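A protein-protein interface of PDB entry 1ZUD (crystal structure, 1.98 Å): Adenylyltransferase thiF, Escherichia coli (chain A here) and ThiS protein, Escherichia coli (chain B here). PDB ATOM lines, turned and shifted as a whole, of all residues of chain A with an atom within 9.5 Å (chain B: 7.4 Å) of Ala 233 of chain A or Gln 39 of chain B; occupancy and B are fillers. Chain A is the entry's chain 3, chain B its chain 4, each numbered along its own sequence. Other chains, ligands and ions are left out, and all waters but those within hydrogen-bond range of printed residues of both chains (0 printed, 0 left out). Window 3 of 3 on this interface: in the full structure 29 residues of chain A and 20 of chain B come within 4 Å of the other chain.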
ATOM      1  N   LEU A 158     -11.035   8.393  31.889  1.00  0.00           N
ATOM      2  CA  LEU A 158     -10.039   7.461  31.377  1.00  0.00           C
ATOM      3  C   LEU A 158      -9.565   7.908  29.945  1.00  0.00           C
ATOM      4  O   LEU A 158     -10.374   8.387  29.159  1.00  0.00           O
ATOM      5  CB  LEU A 158     -10.688   6.076  31.281  1.00  0.00           C
ATOM      6  CG  LEU A 158     -10.000   5.014  30.436  1.00  0.00           C
ATOM      7  CD1 LEU A 158      -8.752   4.577  31.153  1.00  0.00           C
ATOM      8  CD2 LEU A 158     -10.959   3.812  30.234  1.00  0.00           C
ATOM      9  N   MET A 159      -8.275   7.746  29.639  1.00  0.00           N
ATOM     10  CA  MET A 159      -7.755   8.049  28.295  1.00  0.00           C
ATOM     11  C   MET A 159      -6.602   7.129  28.011  1.00  0.00           C
ATOM     12  O   MET A 159      -5.780   6.850  28.921  1.00  0.00           O
ATOM     13  CB  MET A 159      -7.134   9.451  28.183  1.00  0.00           C
ATOM     14  CG  MET A 159      -7.748  10.540  28.905  1.00  0.00           C
ATOM     15  SD  MET A 159      -6.624  11.942  28.594  1.00  0.00           S
ATOM     16  CE  MET A 159      -6.149  12.251  30.222  1.00  0.00           C
ATOM     17  N   LEU A 161      -3.262   7.102  25.764  1.00  0.00           N
ATOM     18  CA  LEU A 161      -2.418   8.023  24.976  1.00  0.00           C
ATOM     19  C   LEU A 161      -1.249   7.235  24.440  1.00  0.00           C
ATOM     20  O   LEU A 161      -0.467   6.602  25.195  1.00  0.00           O
ATOM     21  CB  LEU A 161      -1.915   9.162  25.848  1.00  0.00           C
ATOM     22  CG  LEU A 161      -2.918   9.850  26.720  1.00  0.00           C
ATOM     23  CD1 LEU A 161      -2.184  10.637  27.819  1.00  0.00           C
ATOM     24  CD2 LEU A 161      -3.762  10.729  25.870  1.00  0.00           C
ATOM     25  N   GLU A 166      -0.758  11.627  18.203  1.00  0.00           N
ATOM     26  CA  GLU A 166      -1.591  12.342  17.251  1.00  0.00           C
ATOM     27  C   GLU A 166      -2.660  13.229  17.932  1.00  0.00           C
ATOM     28  O   GLU A 166      -3.019  14.327  17.441  1.00  0.00           O
ATOM     29  CB  GLU A 166      -2.269  11.311  16.336  1.00  0.00           C
ATOM     30  CG  GLU A 166      -1.298  10.520  15.457  1.00  0.00           C
ATOM     31  CD  GLU A 166      -1.971   9.393  14.662  1.00  0.00           C
ATOM     32  OE1 GLU A 166      -3.099   9.596  14.154  1.00  0.00           O
ATOM     33  OE2 GLU A 166      -1.365   8.306  14.531  1.00  0.00           O
ATOM     34  N   GLN A 167      -3.183  12.764  19.069  1.00  0.00           N
ATOM     35  CA  GLN A 167      -4.205  13.532  19.775  1.00  0.00           C
ATOM     36  C   GLN A 167      -3.687  14.255  20.984  1.00  0.00           C
ATOM     37  O   GLN A 167      -4.486  14.633  21.867  1.00  0.00           O
ATOM     38  CB  GLN A 167      -5.404  12.638  20.218  1.00  0.00           C
ATOM     39  CG  GLN A 167      -6.460  12.463  19.125  1.00  0.00           C
ATOM     40  CD  GLN A 167      -5.988  11.555  17.988  1.00  0.00           C
ATOM     41  OE1 GLN A 167      -5.536  10.429  18.215  1.00  0.00           O
ATOM     42  NE2 GLN A 167      -6.094  12.046  16.762  1.00  0.00           N
ATOM     43  N   GLY A 168      -2.360  14.407  21.061  1.00  0.00           N
ATOM     44  CA  GLY A 168      -1.764  15.098  22.176  1.00  0.00           C
ATOM     45  C   GLY A 168      -1.447  14.193  23.371  1.00  0.00           C
ATOM     46  O   GLY A 168      -1.426  12.975  23.283  1.00  0.00           O
ATOM     47  N   LEU A 173      -4.455  18.373  27.482  1.00  0.00           N
ATOM     48  CA  LEU A 173      -5.798  18.491  28.045  1.00  0.00           C
ATOM     49  C   LEU A 173      -5.838  19.274  29.355  1.00  0.00           C
ATOM     50  O   LEU A 173      -6.753  20.056  29.593  1.00  0.00           O
ATOM     51  CB  LEU A 173      -6.350  17.061  28.287  1.00  0.00           C
ATOM     52  CG  LEU A 173      -7.700  16.922  28.988  1.00  0.00           C
ATOM     53  CD1 LEU A 173      -8.762  17.649  28.142  1.00  0.00           C
ATOM     54  CD2 LEU A 173      -8.071  15.395  29.126  1.00  0.00           C
ATOM     55  N   PRO A 215      -9.868   1.953  19.702  1.00  0.00           N
ATOM     56  CA  PRO A 215      -9.554   3.397  19.709  1.00  0.00           C
ATOM     57  C   PRO A 215      -8.595   3.878  20.821  1.00  0.00           C
ATOM     58  O   PRO A 215      -8.405   3.219  21.857  1.00  0.00           O
ATOM     59  CB  PRO A 215     -10.937   4.060  19.799  1.00  0.00           C
ATOM     60  CG  PRO A 215     -11.764   3.024  20.606  1.00  0.00           C
ATOM     61  CD  PRO A 215     -11.297   1.691  20.007  1.00  0.00           C
ATOM     62  N   ALA A 216      -7.957   5.015  20.570  1.00  0.00           N
ATOM     63  CA  ALA A 216      -7.069   5.643  21.536  1.00  0.00           C
ATOM     64  C   ALA A 216      -7.241   7.150  21.291  1.00  0.00           C
ATOM     65  O   ALA A 216      -7.844   7.556  20.275  1.00  0.00           O
ATOM     66  CB  ALA A 216      -5.594   5.174  21.300  1.00  0.00           C
ATOM     67  N   GLY A 217      -6.777   7.994  22.212  1.00  0.00           N
ATOM     68  CA  GLY A 217      -6.905   9.440  22.006  1.00  0.00           C
ATOM     69  C   GLY A 217      -8.330   9.935  22.145  1.00  0.00           C
ATOM     70  O   GLY A 217      -8.791  10.872  21.479  1.00  0.00           O
ATOM     71  N   GLU A 218      -9.015   9.297  23.081  1.00  0.00           N
ATOM     72  CA  GLU A 218     -10.403   9.548  23.377  1.00  0.00           C
ATOM     73  C   GLU A 218     -10.530   9.706  24.906  1.00  0.00           C
ATOM     74  O   GLU A 218     -10.019   8.868  25.624  1.00  0.00           O
ATOM     75  CB  GLU A 218     -11.091   8.282  22.917  1.00  0.00           C
ATOM     76  CG  GLU A 218     -12.536   8.234  22.739  1.00  0.00           C
ATOM     77  CD  GLU A 218     -12.908   6.881  22.103  1.00  0.00           C
ATOM     78  OE1 GLU A 218     -12.566   5.816  22.699  1.00  0.00           O
ATOM     79  OE2 GLU A 218     -13.525   6.892  21.011  1.00  0.00           O
ATOM     80  N   LEU A 219     -11.198  10.749  25.404  1.00  0.00           N
ATOM     81  CA  LEU A 219     -11.379  10.885  26.832  1.00  0.00           C
ATOM     82  C   LEU A 219     -12.760  10.239  27.137  1.00  0.00           C
ATOM     83  O   LEU A 219     -13.755  10.587  26.509  1.00  0.00           O
ATOM     84  CB  LEU A 219     -11.365  12.369  27.259  1.00  0.00           C
ATOM     85  CG  LEU A 219     -11.761  12.625  28.713  1.00  0.00           C
ATOM     86  CD1 LEU A 219     -10.680  12.006  29.625  1.00  0.00           C
ATOM     87  CD2 LEU A 219     -11.925  14.136  28.975  1.00  0.00           C
ATOM     88  N   ARG A 220     -12.775   9.231  28.025  1.00  0.00           N
ATOM     89  CA  ARG A 220     -14.014   8.549  28.382  1.00  0.00           C
ATOM     90  C   ARG A 220     -14.422   8.993  29.793  1.00  0.00           C
ATOM     91  O   ARG A 220     -13.644   8.914  30.726  1.00  0.00           O
ATOM     92  CB  ARG A 220     -13.778   7.048  28.255  1.00  0.00           C
ATOM     93  CG  ARG A 220     -13.612   6.666  26.782  1.00  0.00           C
ATOM     94  CD  ARG A 220     -12.785   5.401  26.571  1.00  0.00           C
ATOM     95  NE  ARG A 220     -13.402   4.235  27.229  1.00  0.00           N
ATOM     96  CZ  ARG A 220     -12.833   3.032  27.313  1.00  0.00           C
ATOM     97  NH1 ARG A 220     -11.626   2.803  26.771  1.00  0.00           N
ATOM     98  NH2 ARG A 220     -13.452   2.059  27.979  1.00  0.00           N
ATOM     99  N   LEU A 221     -15.628   9.504  29.932  1.00  0.00           N
ATOM    100  CA  LEU A 221     -16.097  10.031  31.215  1.00  0.00           C
ATOM    101  C   LEU A 221     -17.277   9.185  31.699  1.00  0.00           C
ATOM    102  O   LEU A 221     -18.193   8.853  30.945  1.00  0.00           O
ATOM    103  CB  LEU A 221     -16.537  11.506  31.082  1.00  0.00           C
ATOM    104  CG  LEU A 221     -15.494  12.451  30.403  1.00  0.00           C
ATOM    105  CD1 LEU A 221     -16.127  13.860  30.197  1.00  0.00           C
ATOM    106  CD2 LEU A 221     -14.241  12.606  31.244  1.00  0.00           C
ATOM    107  N   ARG A 230     -19.623   9.062  28.285  1.00  0.00           N
ATOM    108  CA  ARG A 230     -19.537   9.886  27.055  1.00  0.00           C
ATOM    109  C   ARG A 230     -18.084   9.792  26.632  1.00  0.00           C
ATOM    110  O   ARG A 230     -17.221   9.578  27.480  1.00  0.00           O
ATOM    111  CB  ARG A 230     -19.985  11.314  27.289  1.00  0.00           C
ATOM    112  CG  ARG A 230     -19.170  12.120  28.154  1.00  0.00           C
ATOM    113  CD  ARG A 230     -20.122  13.009  28.966  1.00  0.00           C
ATOM    114  NE  ARG A 230     -21.090  13.620  28.083  1.00  0.00           N
ATOM    115  CZ  ARG A 230     -22.150  14.323  28.472  1.00  0.00           C
ATOM    116  NH1 ARG A 230     -22.412  14.517  29.760  1.00  0.00           N
ATOM    117  NH2 ARG A 230     -22.926  14.847  27.545  1.00  0.00           N
ATOM    118  N   SER A 231     -17.828   9.889  25.322  1.00  0.00           N
ATOM    119  CA  SER A 231     -16.492   9.794  24.757  1.00  0.00           C
ATOM    120  C   SER A 231     -16.220  11.091  24.048  1.00  0.00           C
ATOM    121  O   SER A 231     -17.023  11.507  23.204  1.00  0.00           O
ATOM    122  CB  SER A 231     -16.407   8.646  23.729  1.00  0.00           C
ATOM    123  OG  SER A 231     -16.388   7.381  24.398  1.00  0.00           O
ATOM    124  N   LEU A 232     -15.093  11.716  24.371  1.00  0.00           N
ATOM    125  CA  LEU A 232     -14.730  13.006  23.739  1.00  0.00           C
ATOM    126  C   LEU A 232     -13.412  12.821  22.999  1.00  0.00           C
ATOM    127  O   LEU A 232     -12.498  12.175  23.507  1.00  0.00           O
ATOM    128  CB  LEU A 232     -14.581  14.085  24.819  1.00  0.00           C
ATOM    129  CG  LEU A 232     -15.821  14.188  25.723  1.00  0.00           C
ATOM    130  CD1 LEU A 232     -15.495  15.126  26.910  1.00  0.00           C
ATOM    131  CD2 LEU A 232     -17.037  14.744  24.881  1.00  0.00           C
ATOM    132  N   ALA A 233     -13.319  13.375  21.791  1.00  0.00           N
ATOM    133  CA  ALA A 233     -12.083  13.236  21.015  1.00  0.00           C
ATOM    134  C   ALA A 233     -11.085  14.210  21.590  1.00  0.00           C
ATOM    135  O   ALA A 233     -11.395  15.414  21.695  1.00  0.00           O
ATOM    136  CB  ALA A 233     -12.367  13.582  19.499  1.00  0.00           C
ATOM    137  N   LEU A 234      -9.888  13.725  21.953  1.00  0.00           N
ATOM    138  CA  LEU A 234      -8.851  14.577  22.496  1.00  0.00           C
ATOM    139  C   LEU A 234      -8.275  15.436  21.326  1.00  0.00           C
ATOM    140  O   LEU A 234      -8.530  15.139  20.155  1.00  0.00           O
ATOM    141  CB  LEU A 234      -7.723  13.725  23.109  1.00  0.00           C
ATOM    142  CG  LEU A 234      -8.155  13.040  24.447  1.00  0.00           C
ATOM    143  CD1 LEU A 234      -7.114  12.036  24.895  1.00  0.00           C
ATOM    144  CD2 LEU A 234      -8.336  14.136  25.497  1.00  0.00           C
ATOM    145  N   ARG A 235      -7.518  16.475  21.646  1.00  0.00           N
ATOM    146  CA  ARG A 235      -6.923  17.304  20.564  1.00  0.00           C
ATOM    147  C   ARG A 235      -5.603  17.859  21.067  1.00  0.00           C
ATOM    148  O   ARG A 235      -5.539  18.439  22.149  1.00  0.00           O
ATOM    149  CB  ARG A 235      -7.852  18.485  20.221  1.00  0.00           C
ATOM    150  CG  ARG A 235      -7.286  19.497  19.186  1.00  0.00           C
ATOM    151  CD  ARG A 235      -7.585  19.101  17.719  1.00  0.00           C
ATOM    152  NE  ARG A 235      -6.958  20.005  16.731  1.00  0.00           N
ATOM    153  CZ  ARG A 235      -5.722  19.872  16.223  1.00  0.00           C
ATOM    154  NH1 ARG A 235      -4.931  18.862  16.584  1.00  0.00           N
ATOM    155  NH2 ARG A 235      -5.261  20.762  15.343  1.00  0.00           N
ATOM    156  N   ARG A 236      -4.536  17.695  20.305  1.00  0.00           N
ATOM    157  CA  ARG A 236      -3.283  18.220  20.790  1.00  0.00           C
ATOM    158  C   ARG A 236      -3.276  19.737  20.836  1.00  0.00           C
ATOM    159  O   ARG A 236      -4.030  20.417  20.129  1.00  0.00           O
ATOM    160  CB  ARG A 236      -2.098  17.638  19.999  1.00  0.00           C
ATOM    161  CG  ARG A 236      -2.067  17.932  18.558  1.00  0.00           C
ATOM    162  CD  ARG A 236      -0.746  17.441  17.947  1.00  0.00           C
ATOM    163  NE  ARG A 236      -0.685  17.912  16.569  1.00  0.00           N
ATOM    164  CZ  ARG A 236      -1.210  17.283  15.517  1.00  0.00           C
ATOM    165  NH1 ARG A 236      -1.845  16.113  15.656  1.00  0.00           N
ATOM    166  NH2 ARG A 236      -1.115  17.849  14.314  1.00  0.00           N
ATOM    167  N   LEU B  34     -12.916  21.808  28.179  1.00  0.00           N
ATOM    168  CA  LEU B  34     -14.142  22.082  27.454  1.00  0.00           C
ATOM    169  C   LEU B  34     -14.209  21.282  26.130  1.00  0.00           C
ATOM    170  O   LEU B  34     -13.194  21.099  25.431  1.00  0.00           O
ATOM    171  CB  LEU B  34     -14.211  23.619  27.198  1.00  0.00           C
ATOM    172  CG  LEU B  34     -15.490  24.066  26.482  1.00  0.00           C
ATOM    173  CD1 LEU B  34     -16.212  25.070  27.358  1.00  0.00           C
ATOM    174  CD2 LEU B  34     -15.179  24.603  25.098  1.00  0.00           C
ATOM    175  N   ALA B  35     -15.396  20.774  25.809  1.00  0.00           N
ATOM    176  CA  ALA B  35     -15.586  20.077  24.554  1.00  0.00           C
ATOM    177  C   ALA B  35     -16.693  20.800  23.787  1.00  0.00           C
ATOM    178  O   ALA B  35     -17.641  21.339  24.394  1.00  0.00           O
ATOM    179  CB  ALA B  35     -16.007  18.655  24.784  1.00  0.00           C
ATOM    180  N   ILE B  36     -16.568  20.844  22.466  1.00  0.00           N
ATOM    181  CA  ILE B  36     -17.646  21.444  21.661  1.00  0.00           C
ATOM    182  C   ILE B  36     -17.966  20.393  20.652  1.00  0.00           C
ATOM    183  O   ILE B  36     -17.070  19.937  19.939  1.00  0.00           O
ATOM    184  CB  ILE B  36     -17.222  22.771  20.938  1.00  0.00           C
ATOM    185  CG1 ILE B  36     -17.150  23.884  21.976  1.00  0.00           C
ATOM    186  CG2 ILE B  36     -18.274  23.160  19.818  1.00  0.00           C
ATOM    187  CD1 ILE B  36     -16.662  25.268  21.395  1.00  0.00           C
ATOM    188  N   ASN B  37     -19.237  19.981  20.607  1.00  0.00           N
ATOM    189  CA  ASN B  37     -19.616  18.955  19.664  1.00  0.00           C
ATOM    190  C   ASN B  37     -18.730  17.731  19.809  1.00  0.00           C
ATOM    191  O   ASN B  37     -18.233  17.183  18.840  1.00  0.00           O
ATOM    192  CB  ASN B  37     -19.557  19.505  18.245  1.00  0.00           C
ATOM    193  CG  ASN B  37     -20.527  20.657  18.063  1.00  0.00           C
ATOM    194  OD1 ASN B  37     -21.548  20.713  18.750  1.00  0.00           O
ATOM    195  ND2 ASN B  37     -20.209  21.591  17.162  1.00  0.00           N
ATOM    196  N   GLN B  38     -18.510  17.340  21.059  1.00  0.00           N
ATOM    197  CA  GLN B  38     -17.732  16.141  21.349  1.00  0.00           C
ATOM    198  C   GLN B  38     -16.235  16.124  21.056  1.00  0.00           C
ATOM    199  O   GLN B  38     -15.617  15.070  21.031  1.00  0.00           O
ATOM    200  CB  GLN B  38     -18.443  14.929  20.728  1.00  0.00           C
ATOM    201  CG  GLN B  38     -19.875  14.700  21.316  1.00  0.00           C
ATOM    202  CD  GLN B  38     -20.957  15.650  20.752  1.00  0.00           C
ATOM    203  OE1 GLN B  38     -21.093  15.837  19.516  1.00  0.00           O
ATOM    204  NE2 GLN B  38     -21.744  16.243  21.659  1.00  0.00           N
ATOM    205  N   GLN B  39     -15.637  17.299  20.878  1.00  0.00           N
ATOM    206  CA  GLN B  39     -14.191  17.365  20.626  1.00  0.00           C
ATOM    207  C   GLN B  39     -13.643  18.370  21.618  1.00  0.00           C
ATOM    208  O   GLN B  39     -14.193  19.447  21.820  1.00  0.00           O
ATOM    209  CB  GLN B  39     -13.932  17.787  19.170  1.00  0.00           C
ATOM    210  CG  GLN B  39     -15.068  17.394  18.168  1.00  0.00           C
ATOM    211  CD  GLN B  39     -15.018  15.954  17.599  1.00  0.00           C
ATOM    212  OE1 GLN B  39     -14.006  15.511  17.036  1.00  0.00           O
ATOM    213  NE2 GLN B  39     -16.140  15.237  17.716  1.00  0.00           N
ATOM    214  N   ILE B  40     -12.579  17.992  22.285  1.00  0.00           N
ATOM    215  CA  ILE B  40     -11.949  18.903  23.220  1.00  0.00           C
ATOM    216  C   ILE B  40     -11.416  20.125  22.454  1.00  0.00           C
ATOM    217  O   ILE B  40     -10.889  19.981  21.364  1.00  0.00           O
ATOM    218  CB  ILE B  40     -10.725  18.248  23.877  1.00  0.00           C
ATOM    219  CG1 ILE B  40     -11.199  17.004  24.672  1.00  0.00           C
ATOM    220  CG2 ILE B  40      -9.990  19.286  24.781  1.00  0.00           C
ATOM    221  CD1 ILE B  40     -12.037  17.364  25.893  1.00  0.00           C
ATOM    222  N   VAL B  41     -11.554  21.286  23.066  1.00  0.00           N
ATOM    223  CA  VAL B  41     -11.031  22.540  22.552  1.00  0.00           C
ATOM    224  C   VAL B  41      -9.957  22.916  23.595  1.00  0.00           C
ATOM    225  O   VAL B  41     -10.286  23.290  24.712  1.00  0.00           O
ATOM    226  CB  VAL B  41     -12.083  23.667  22.506  1.00  0.00           C
ATOM    227  CG1 VAL B  41     -11.384  24.946  21.985  1.00  0.00           C
ATOM    228  CG2 VAL B  41     -13.217  23.307  21.555  1.00  0.00           C
ATOM    229  N   PRO B  42      -8.671  22.777  23.250  1.00  0.00           N
ATOM    230  CA  PRO B  42      -7.590  23.107  24.185  1.00  0.00           C
ATOM    231  C   PRO B  42      -7.771  24.518  24.769  1.00  0.00           C
ATOM    232  O   PRO B  42      -8.086  25.464  24.065  1.00  0.00           O
ATOM    233  CB  PRO B  42      -6.332  22.958  23.328  1.00  0.00           C
ATOM    234  CG  PRO B  42      -6.698  21.934  22.317  1.00  0.00           C
ATOM    235  CD  PRO B  42      -8.116  22.359  21.929  1.00  0.00           C
ATOM    236  N   GLN B  56     -22.814  22.182  20.966  1.00  0.00           N
ATOM    237  CA  GLN B  56     -23.140  21.423  22.198  1.00  0.00           C
ATOM    238  C   GLN B  56     -21.876  21.493  23.034  1.00  0.00           C
ATOM    239  O   GLN B  56     -20.837  20.943  22.679  1.00  0.00           O
ATOM    240  CB  GLN B  56     -23.520  19.977  21.876  1.00  0.00           C
ATOM    241  CG  GLN B  56     -24.574  19.884  20.779  1.00  0.00           C
ATOM    242  CD  GLN B  56     -25.133  18.493  20.672  1.00  0.00           C
ATOM    243  OE1 GLN B  56     -24.386  17.523  20.683  1.00  0.00           O
ATOM    244  NE2 GLN B  56     -26.452  18.384  20.568  1.00  0.00           N
ATOM    245  N   LEU B  58     -19.659  21.225  26.695  1.00  0.00           N
ATOM    246  CA  LEU B  58     -19.495  20.569  28.005  1.00  0.00           C
ATOM    247  C   LEU B  58     -18.315  21.241  28.676  1.00  0.00           C
ATOM    248  O   LEU B  58     -17.245  21.422  28.075  1.00  0.00           O
ATOM    249  CB  LEU B  58     -19.130  19.091  27.845  1.00  0.00           C
ATOM    250  CG  LEU B  58     -20.082  18.211  27.062  1.00  0.00           C
ATOM    251  CD1 LEU B  58     -19.596  16.774  27.170  1.00  0.00           C
ATOM    252  CD2 LEU B  58     -21.519  18.349  27.651  1.00  0.00           C
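Printed residues of chain B within 4 Å of Ala 233 of chain A: Gln 38, Gln 39 and Ile 40.
Of the printed residues of chain A, Gln 39 of chain B touches Ala 233.
No residue of chain A comes within 4 Å of Ala 35 of chain B.
Of the printed residues of chain B, Leu 173 of chain A touches Ile 40 (3.9 Å).
Of the printed residues of chain B, Arg 236 of chain A touches Pro 42 (3.8 Å).
Printed residues of chain B within 4 Å of Leu 232 of chain A: Gln 38 (3.5 Å) and Leu 58 (3.99 Å).
Printed residues of chain A within 4 Å of Ile 40 of chain B: Leu 173, Ala 233 and Arg 235.
The nearest printed residue of chain B that does not touch Ala 233 of chain A is Val 41 of chain B (6.0 Å).
The nearest printed residue of chain A that does not touch Gln 39 of chain B is Leu 232 of chain A (5.0 Å).
Hydrophobic or aromatic side chains of chain B within 4 Å of the printed part of chain A: Ile 40, Pro 42 and Leu 58.
Hydrophobic or aromatic side chains of chain A that line the printed part of chain B: Leu 173, Leu 232 and Ala 233.
Among the printed residues, 10 pairs touch across the chains.
Among the printed residues, no Asp or Glu carboxylate lies within 4 Å of a Lys or Arg side-chain nitrogen of the other chain.
The backbone NH (N) of Ala 233 of chain A is in hydrogen-bond range of the backbone carbonyl oxygen (O) of Gln 38 of chain B (3.0 Å).
The backbone carbonyl oxygen (O) of Ala 233 of chain A lies within hydrogen-bond range of the backbone NH (N) of Ile 40 of chain B, at 2.9 Å.
CD1 of Leu 173 of chain A touches CG2 of Ile 40 of chain B, at 3.9 Å.
Leu 58 of chain B touches Arg 230 of chain A.
Leu 232 of chain A touches Gln 38 of chain B.
CD2 of Leu 232 of chain A touches CD1 of Leu 58 of chain B, 3.99 Å away.
Gln 39 of chain B touches Ala 233 of chain A (OE1 to CB, 3.5 Å).
CB of Arg 235 of chain A touches O of Ile 40 of chain B, 3.6 Å away.
Arg 235 of chain A touches Pro 42 of chain B (O to CG, 3.7 Å).
Arg 236 of chain A touches Pro 42 of chain B.
NH1 of Arg 236 of chain A is in hydrogen-bond range of O of Glu 166 of chain A (2.8 Å).
O of Gln 167 of chain A lies within hydrogen-bond range of N of Arg 236 of chain A.
N of Leu 219 of chain A is in hydrogen-bond range of O of Leu 232 of chain A (2.7 Å).
The backbone carbonyl oxygen (O) of Leu 58 of chain B is in hydrogen-bond range of the backbone NH (N) of Ala 35 of chain B (3.0 Å).
NE2 of Gln 39 of chain B is in hydrogen-bond range of O of Asn 37 of chain B (3.1 Å).
NE2 of Gln 38 of chain B lies within hydrogen-bond range of OE1 of Gln 56 of chain B (3.1 Å).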
